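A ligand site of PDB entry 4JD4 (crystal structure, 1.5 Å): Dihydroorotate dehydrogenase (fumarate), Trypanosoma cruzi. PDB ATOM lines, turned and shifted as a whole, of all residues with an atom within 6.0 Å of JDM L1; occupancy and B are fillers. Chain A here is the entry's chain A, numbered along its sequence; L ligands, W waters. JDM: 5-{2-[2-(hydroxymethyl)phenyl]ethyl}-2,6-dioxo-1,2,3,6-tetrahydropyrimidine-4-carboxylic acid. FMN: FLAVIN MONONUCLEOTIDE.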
ATOM      1  N   LYS A  44       4.921 -12.026  10.778  1.00  0.00           N
ATOM      2  CA  LYS A  44       5.569 -12.382  12.031  1.00  0.00           C
ATOM      3  C   LYS A  44       4.820 -13.580  12.612  1.00  0.00           C
ATOM      4  O   LYS A  44       3.563 -13.551  12.692  1.00  0.00           O
ATOM      5  CB  LYS A  44       5.470 -11.188  13.010  1.00  0.00           C
ATOM      6  CG  LYS A  44       5.810 -11.466  14.445  1.00  0.00           C
ATOM      7  CD  LYS A  44       7.297 -11.735  14.734  1.00  0.00           C
ATOM      8  CE  LYS A  44       7.671 -12.309  16.108  1.00  0.00           C
ATOM      9  NZ  LYS A  44       9.161 -12.707  16.266  1.00  0.00           N
ATOM     10  N   SER A  45       5.520 -14.540  13.166  1.00  0.00           N
ATOM     11  CA  SER A  45       4.856 -15.692  13.848  1.00  0.00           C
ATOM     12  C   SER A  45       3.994 -15.099  14.964  1.00  0.00           C
ATOM     13  O   SER A  45       4.417 -14.279  15.776  1.00  0.00           O
ATOM     14  CB  SER A  45       5.789 -16.635  14.516  1.00  0.00           C
ATOM     15  OG  SER A  45       6.603 -17.331  13.520  1.00  0.00           O
ATOM     16  N   THR A  47       0.646 -15.467  17.972  1.00  0.00           N
ATOM     17  CA  THR A  47      -0.081 -16.172  19.003  1.00  0.00           C
ATOM     18  C   THR A  47      -1.517 -15.664  18.922  1.00  0.00           C
ATOM     19  O   THR A  47      -1.842 -14.617  18.352  1.00  0.00           O
ATOM     20  CB  THR A  47       0.562 -15.897  20.394  1.00  0.00           C
ATOM     21  OG1 THR A  47       0.839 -14.523  20.572  1.00  0.00           O
ATOM     22  CG2 THR A  47       1.775 -16.754  20.705  1.00  0.00           C
ATOM     23  N   ARG A  51       1.348 -10.048  22.048  1.00  0.00           N
ATOM     24  CA  ARG A  51       2.432 -10.145  23.033  1.00  0.00           C
ATOM     25  C   ARG A  51       3.361  -8.950  22.929  1.00  0.00           C
ATOM     26  O   ARG A  51       3.721  -8.511  21.800  1.00  0.00           O
ATOM     27  CB  ARG A  51       3.262 -11.373  22.805  1.00  0.00           C
ATOM     28  CG  ARG A  51       2.618 -12.676  22.967  1.00  0.00           C
ATOM     29  CD  ARG A  51       3.445 -13.885  22.617  1.00  0.00           C
ATOM     30  NE  ARG A  51       4.728 -13.962  23.266  1.00  0.00           N
ATOM     31  CZ  ARG A  51       4.990 -14.681  24.344  1.00  0.00           C
ATOM     32  NH1 ARG A  51       4.010 -15.357  24.967  1.00  0.00           N
ATOM     33  NH2 ARG A  51       6.200 -14.704  24.862  1.00  0.00           N
ATOM     34  N   ASN A  54       9.987  -9.726  25.038  1.00  0.00           N
ATOM     35  CA  ASN A  54      10.899  -9.573  26.111  1.00  0.00           C
ATOM     36  C   ASN A  54      11.405  -8.181  26.218  1.00  0.00           C
ATOM     37  O   ASN A  54      11.309  -7.335  25.332  1.00  0.00           O
ATOM     38  CB  ASN A  54      12.067 -10.529  25.827  1.00  0.00           C
ATOM     39  CG  ASN A  54      11.748 -11.945  26.016  1.00  0.00           C
ATOM     40  OD1 ASN A  54      10.812 -12.315  26.780  1.00  0.00           O
ATOM     41  ND2 ASN A  54      12.499 -12.799  25.449  1.00  0.00           N
ATOM     42  N   ASN A  68      19.289 -12.879  18.936  1.00  0.00           N
ATOM     43  CA  ASN A  68      17.988 -12.375  19.366  1.00  0.00           C
ATOM     44  C   ASN A  68      17.323 -13.311  20.318  1.00  0.00           C
ATOM     45  O   ASN A  68      17.355 -14.504  20.252  1.00  0.00           O
ATOM     46  CB  ASN A  68      17.042 -12.079  18.185  1.00  0.00           C
ATOM     47  CG  ASN A  68      16.221 -13.255  17.795  1.00  0.00           C
ATOM     48  OD1 ASN A  68      15.141 -13.562  18.369  1.00  0.00           O
ATOM     49  ND2 ASN A  68      16.670 -13.951  16.760  1.00  0.00           N
ATOM     50  N   SER A  69      16.620 -12.599  21.295  1.00  0.00           N
ATOM     51  CA  SER A  69      15.635 -13.250  22.184  1.00  0.00           C
ATOM     52  C   SER A  69      14.410 -12.407  22.257  1.00  0.00           C
ATOM     53  O   SER A  69      14.186 -11.758  23.272  1.00  0.00           O
ATOM     54  CB  SER A  69      16.198 -13.645  23.523  1.00  0.00           C
ATOM     55  OG  SER A  69      17.106 -14.827  23.414  1.00  0.00           O
ATOM     56  N   MET A  70      13.698 -12.296  21.144  1.00  0.00           N
ATOM     57  CA  MET A  70      12.639 -11.282  21.010  1.00  0.00           C
ATOM     58  C   MET A  70      11.511 -11.624  21.956  1.00  0.00           C
ATOM     59  O   MET A  70      10.874 -10.683  22.466  1.00  0.00           O
ATOM     60  CB  MET A  70      12.139 -11.188  19.589  1.00  0.00           C
ATOM     61  CG  MET A  70      13.090 -10.869  18.500  1.00  0.00           C
ATOM     62  SD  MET A  70      13.921  -9.303  18.683  1.00  0.00           S
ATOM     63  CE  MET A  70      12.711  -8.174  18.291  1.00  0.00           C
ATOM     64  N   GLY A  71      11.197 -12.885  22.159  1.00  0.00           N
ATOM     65  CA  GLY A  71      10.060 -13.301  22.983  1.00  0.00           C
ATOM     66  C   GLY A  71       8.747 -13.243  22.281  1.00  0.00           C
ATOM     67  O   GLY A  71       7.683 -13.141  22.894  1.00  0.00           O
ATOM     68  N   LEU A  72       8.787 -13.392  20.959  1.00  0.00           N
ATOM     69  CA  LEU A  72       7.587 -13.413  20.120  1.00  0.00           C
ATOM     70  C   LEU A  72       6.692 -12.205  20.295  1.00  0.00           C
ATOM     71  O   LEU A  72       5.455 -12.376  20.441  1.00  0.00           O
ATOM     72  CB  LEU A  72       6.819 -14.748  20.197  1.00  0.00           C
ATOM     73  CG  LEU A  72       5.966 -14.938  18.942  1.00  0.00           C
ATOM     74  CD1 LEU A  72       6.742 -15.667  17.860  1.00  0.00           C
ATOM     75  CD2 LEU A  72       4.716 -15.706  19.164  1.00  0.00           C
ATOM     76  N   PRO A  73       7.212 -10.992  20.248  1.00  0.00           N
ATOM     77  CA  PRO A  73       6.357  -9.796  20.181  1.00  0.00           C
ATOM     78  C   PRO A  73       5.544  -9.872  18.937  1.00  0.00           C
ATOM     79  O   PRO A  73       6.092 -10.071  17.844  1.00  0.00           O
ATOM     80  CB  PRO A  73       7.317  -8.618  20.166  1.00  0.00           C
ATOM     81  CG  PRO A  73       8.604  -9.204  19.643  1.00  0.00           C
ATOM     82  CD  PRO A  73       8.633 -10.677  19.870  1.00  0.00           C
ATOM     83  N   SER A 100       2.758 -19.522  15.647  1.00  0.00           N
ATOM     84  CA  SER A 100       3.556 -20.167  16.689  1.00  0.00           C
ATOM     85  C   SER A 100       2.852 -20.077  18.019  1.00  0.00           C
ATOM     86  O   SER A 100       3.331 -19.480  18.931  1.00  0.00           O
ATOM     87  CB  SER A 100       5.011 -19.683  16.716  1.00  0.00           C
ATOM     88  OG  SER A 100       5.869 -20.758  17.135  1.00  0.00           O
ATOM     89  N   GLY A 101       1.784 -20.847  18.117  1.00  0.00           N
ATOM     90  CA  GLY A 101       1.079 -20.918  19.405  1.00  0.00           C
ATOM     91  C   GLY A 101       1.890 -21.635  20.460  1.00  0.00           C
ATOM     92  O   GLY A 101       2.798 -22.436  20.189  1.00  0.00           O
ATOM     93  N   LEU A 102       1.497 -21.415  21.762  1.00  0.00           N
ATOM     94  CA  LEU A 102       2.206 -21.959  22.936  1.00  0.00           C
ATOM     95  C   LEU A 102       1.696 -23.334  23.332  1.00  0.00           C
ATOM     96  O   LEU A 102       2.294 -23.932  24.226  1.00  0.00           O
ATOM     97  CB  LEU A 102       2.033 -21.028  24.136  1.00  0.00           C
ATOM     98  CG  LEU A 102       2.316 -19.525  23.902  1.00  0.00           C
ATOM     99  CD1 LEU A 102       2.203 -18.681  25.179  1.00  0.00           C
ATOM    100  CD2 LEU A 102       3.620 -19.250  23.260  1.00  0.00           C
ATOM    101  N   ASN A 128       5.467 -22.511  12.688  1.00  0.00           N
ATOM    102  CA  ASN A 128       6.778 -22.412  13.347  1.00  0.00           C
ATOM    103  C   ASN A 128       6.875 -23.388  14.477  1.00  0.00           C
ATOM    104  O   ASN A 128       6.227 -23.202  15.531  1.00  0.00           O
ATOM    105  CB  ASN A 128       6.994 -20.986  13.835  1.00  0.00           C
ATOM    106  CG  ASN A 128       8.273 -20.778  14.597  1.00  0.00           C
ATOM    107  OD1 ASN A 128       9.048 -21.651  14.736  1.00  0.00           O
ATOM    108  ND2 ASN A 128       8.472 -19.542  15.067  1.00  0.00           N
ATOM    109  N   SER A 130       9.468 -24.163  16.295  1.00  0.00           N
ATOM    110  CA  SER A 130      10.374 -23.763  17.380  1.00  0.00           C
ATOM    111  C   SER A 130       9.610 -23.055  18.465  1.00  0.00           C
ATOM    112  O   SER A 130       9.904 -21.970  18.820  1.00  0.00           O
ATOM    113  CB  SER A 130      11.507 -22.871  16.888  1.00  0.00           C
ATOM    114  OG  SER A 130      12.356 -23.683  16.136  1.00  0.00           O
ATOM    115  N   CYS A 131       8.555 -23.655  18.921  1.00  0.00           N
ATOM    116  CA  CYS A 131       7.562 -23.090  19.848  1.00  0.00           C
ATOM    117  C   CYS A 131       7.715 -23.888  21.154  1.00  0.00           C
ATOM    118  O   CYS A 131       8.305 -25.043  21.222  1.00  0.00           O
ATOM    119  CB  CYS A 131       6.143 -23.157  19.270  1.00  0.00           C
ATOM    120  SG  CYS A 131       5.726 -24.803  18.575  1.00  0.00           S
ATOM    121  N   PRO A 132       7.199 -23.300  22.224  1.00  0.00           N
ATOM    122  CA  PRO A 132       7.553 -23.954  23.473  1.00  0.00           C
ATOM    123  C   PRO A 132       6.714 -25.209  23.695  1.00  0.00           C
ATOM    124  O   PRO A 132       5.609 -25.468  23.139  1.00  0.00           O
ATOM    125  CB  PRO A 132       7.266 -22.876  24.551  1.00  0.00           C
ATOM    126  CG  PRO A 132       6.315 -21.914  23.897  1.00  0.00           C
ATOM    127  CD  PRO A 132       6.813 -21.880  22.451  1.00  0.00           C
ATOM    128  N   LYS A 165       8.313 -24.441   9.589  1.00  0.00           N
ATOM    129  CA  LYS A 165       9.588 -23.831   9.843  1.00  0.00           C
ATOM    130  C   LYS A 165      10.284 -24.669  10.917  1.00  0.00           C
ATOM    131  O   LYS A 165       9.771 -24.839  12.019  1.00  0.00           O
ATOM    132  CB  LYS A 165       9.375 -22.426  10.289  1.00  0.00           C
ATOM    133  CG  LYS A 165      10.584 -21.595  10.675  1.00  0.00           C
ATOM    134  CD  LYS A 165      11.371 -21.161   9.513  1.00  0.00           C
ATOM    135  CE  LYS A 165      12.497 -20.158   9.818  1.00  0.00           C
ATOM    136  NZ  LYS A 165      11.957 -18.847  10.131  1.00  0.00           N
ATOM    137  N   ASN A 195      15.369 -22.046  11.138  1.00  0.00           N
ATOM    138  CA  ASN A 195      15.296 -21.053  12.214  1.00  0.00           C
ATOM    139  C   ASN A 195      16.684 -20.730  12.761  1.00  0.00           C
ATOM    140  O   ASN A 195      17.687 -21.343  12.364  1.00  0.00           O
ATOM    141  CB  ASN A 195      14.281 -21.548  13.270  1.00  0.00           C
ATOM    142  CG  ASN A 195      13.508 -20.398  13.889  1.00  0.00           C
ATOM    143  OD1 ASN A 195      14.104 -19.378  14.279  1.00  0.00           O
ATOM    144  ND2 ASN A 195      12.213 -20.555  14.029  1.00  0.00           N
ATOM    145  N   SER A 196      16.808 -19.743  13.628  1.00  0.00           N
ATOM    146  CA  SER A 196      18.048 -19.388  14.249  1.00  0.00           C
ATOM    147  C   SER A 196      18.672 -20.588  14.964  1.00  0.00           C
ATOM    148  O   SER A 196      18.035 -21.583  15.419  1.00  0.00           O
ATOM    149  CB  SER A 196      17.808 -18.162  15.135  1.00  0.00           C
ATOM    150  OG  SER A 196      16.883 -18.429  16.155  1.00  0.00           O
ATOM    151  N   GLY A 220      19.079 -16.707  19.870  1.00  0.00           N
ATOM    152  CA  GLY A 220      19.280 -17.418  18.633  1.00  0.00           C
ATOM    153  C   GLY A 220      20.165 -16.632  17.723  1.00  0.00           C
ATOM    154  O   GLY A 220      20.075 -15.402  17.571  1.00  0.00           O
HETATM  155  OAJ JDM L   1      10.535 -14.044  18.627  1.00  0.00           O
HETATM  156  CAI JDM L   1      11.534 -14.796  18.952  1.00  0.00           C
HETATM  157  OAK JDM L   1      12.391 -14.773  19.911  1.00  0.00           O
HETATM  158  C4  JDM L   1      11.994 -15.718  17.900  1.00  0.00           C
HETATM  159  N3  JDM L   1      13.321 -15.620  17.447  1.00  0.00           N
HETATM  160  C2  JDM L   1      13.824 -16.553  16.487  1.00  0.00           C
HETATM  161  O2  JDM L   1      15.038 -16.337  16.111  1.00  0.00           O
HETATM  162  N1  JDM L   1      13.036 -17.563  16.018  1.00  0.00           N
HETATM  163  C6  JDM L   1      11.738 -17.732  16.484  1.00  0.00           C
HETATM  164  O6  JDM L   1      11.134 -18.686  16.028  1.00  0.00           O
HETATM  165  C5  JDM L   1      11.259 -16.851  17.486  1.00  0.00           C
HETATM  166  CAL JDM L   1       9.907 -17.145  18.076  1.00  0.00           C
HETATM  167  CAM JDM L   1      10.019 -18.371  19.073  1.00  0.00           C
HETATM  168  CAN JDM L   1       8.837 -18.464  19.968  1.00  0.00           C
HETATM  169  CAO JDM L   1       7.699 -19.135  19.471  1.00  0.00           C
HETATM  170  CAP JDM L   1       6.518 -19.257  20.214  1.00  0.00           C
HETATM  171  CAQ JDM L   1       6.473 -18.587  21.421  1.00  0.00           C
HETATM  172  CAR JDM L   1       7.566 -18.003  21.949  1.00  0.00           C
HETATM  173  CAS JDM L   1       8.782 -17.867  21.230  1.00  0.00           C
HETATM  174  CAT JDM L   1       9.856 -17.105  21.752  1.00  0.00           C
HETATM  175  OAU JDM L   1      10.706 -17.791  22.566  1.00  0.00           O
HETATM  176  N1  FMN L   2      11.580 -17.152  12.860  1.00  0.00           N
HETATM  177  C2  FMN L   2      10.283 -17.525  12.882  1.00  0.00           C
HETATM  178  O2  FMN L   2       9.951 -18.534  12.232  1.00  0.00           O
HETATM  179  N3  FMN L   2       9.347 -16.705  13.424  1.00  0.00           N
HETATM  180  C4  FMN L   2       9.626 -15.581  14.054  1.00  0.00           C
HETATM  181  O4  FMN L   2       8.746 -14.837  14.514  1.00  0.00           O
HETATM  182  C4A FMN L   2      11.005 -15.140  14.074  1.00  0.00           C
HETATM  183  N5  FMN L   2      11.369 -13.973  14.680  1.00  0.00           N
HETATM  184  C5A FMN L   2      12.620 -13.521  14.409  1.00  0.00           C
HETATM  185  C6  FMN L   2      12.962 -12.255  14.835  1.00  0.00           C
HETATM  186  C7  FMN L   2      14.208 -11.735  14.633  1.00  0.00           C
HETATM  187  C7M FMN L   2      14.631 -10.357  15.101  1.00  0.00           C
HETATM  188  C8  FMN L   2      15.227 -12.486  13.981  1.00  0.00           C
HETATM  189  C8M FMN L   2      16.645 -12.048  13.721  1.00  0.00           C
HETATM  190  C9  FMN L   2      14.885 -13.766  13.554  1.00  0.00           C
HETATM  191  C9A FMN L   2      13.610 -14.308  13.753  1.00  0.00           C
HETATM  192  N10 FMN L   2      13.262 -15.574  13.343  1.00  0.00           N
HETATM  193  C10 FMN L   2      11.961 -15.998  13.416  1.00  0.00           C
HETATM  194  C1' FMN L   2      14.183 -16.424  12.674  1.00  0.00           C
HETATM  195  C2' FMN L   2      14.426 -16.044  11.218  1.00  0.00           C
HETATM  196  O2' FMN L   2      13.216 -16.252  10.454  1.00  0.00           O
HETATM  197  C3' FMN L   2      15.455 -16.857  10.518  1.00  0.00           C
HETATM  198  O3' FMN L   2      15.114 -18.246  10.550  1.00  0.00           O
HETATM  199  C4' FMN L   2      16.858 -16.722  11.172  1.00  0.00           C
HETATM  200  O4' FMN L   2      17.111 -15.313  11.532  1.00  0.00           O
HETATM  201  C5' FMN L   2      17.973 -17.230  10.244  1.00  0.00           C
HETATM  202  O5' FMN L   2      18.047 -16.469   9.016  1.00  0.00           O
HETATM  203  P   FMN L   2      19.210 -15.355   8.821  1.00  0.00           P
HETATM  204  O1P FMN L   2      20.555 -16.014   8.928  1.00  0.00           O
HETATM  205  O2P FMN L   2      18.993 -14.342   9.907  1.00  0.00           O
HETATM  206  O3P FMN L   2      18.924 -14.790   7.481  1.00  0.00           O
HETATM  207  O   HOH W   1      12.990 -15.403  23.190  1.00  0.00           O
HETATM  208  O   HOH W   2      14.075 -16.686  20.857  1.00  0.00           O
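An oxygen (OAJ) of JDM L1 lies within hydrogen-bond range of the backbone NH (N) of Leu 72. The side-chain amino group (NZ) of Lys 165 is in hydrogen-bond range of an oxygen (O2') of FMN L2 (2.9 Å). The side-chain amide oxygen (OD1) of Asn 68 lies within hydrogen-bond range of a nitrogen (N3) of JDM L1 (2.9 Å). The side-chain amide oxygen of Asn 195 is in hydrogen-bond range of a nitrogen (N1) of JDM L1 (2.7 Å). The backbone NH of Gly 71 lies within hydrogen-bond range of an oxygen (OAK) of JDM L1 (3.2 Å). The side-chain amide nitrogen (ND2) of Asn 128 is in hydrogen-bond range of an oxygen (O2) of FMN L2 (3.4 Å). The side-chain amino group (NZ) of Lys 44 is in hydrogen-bond range of an oxygen (O4) of FMN L2 (2.8 Å). A nitrogen (N3) of FMN L2 lies within hydrogen-bond range of the side-chain hydroxyl of Ser 45, at 2.8 Å. NZ of Lys 44 is in salt-bridge range of OAJ of JDM L1, at 3.0 Å. The side-chain amide nitrogen (ND2) of Asn 128 is in hydrogen-bond range of an oxygen (O6) of JDM L1 (3.0 Å). An oxygen (O2) of JDM L1 is in hydrogen-bond range of the side-chain hydroxyl (OG) of Ser 196, at 2.8 Å. N of Met 70 lies within hydrogen-bond range of OAK of JDM L1, 3.1 Å away.
The backbone carbonyl oxygen of Met 70 is in hydrogen-bond range of the backbone NH of Asn 54 (2.9 Å). ND2 of Asn 128 lies within hydrogen-bond range of OG of Ser 45, at 3.3 Å. The side-chain amide oxygen (OD1) of Asn 195 lies within hydrogen-bond range of the side-chain hydroxyl (OG) of Ser 196, at 3.5 Å. The side-chain amide oxygen (OD1) of Asn 68 sits at hydrogen-bond distance from the backbone NH (N) of Met 70. O of Asn 128 sits at hydrogen-bond distance from SG of Cys 131 (3.5 Å). The backbone carbonyl oxygen of Asn 128 lies within hydrogen-bond range of the side-chain hydroxyl of Ser 100 (2.9 Å). The backbone carbonyl oxygen (O) of Leu 72 lies within hydrogen-bond range of the guanidinium group (NE) of Arg 51 (3.3 Å). The side-chain amide oxygen (OD1) of Asn 128 lies within hydrogen-bond range of the backbone NH (N) of Ser 130.
Residues that only touch JDM L1: Ser 69, Ser 100, Leu 102, Ser 130, Cys 131 and Pro 132.
Water W1 lies within hydrogen-bond range of N of Gly 71 (3.3 Å), OAU of JDM L1 (3.4 Å) and ND2 of Asn 54 (3.5 Å).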
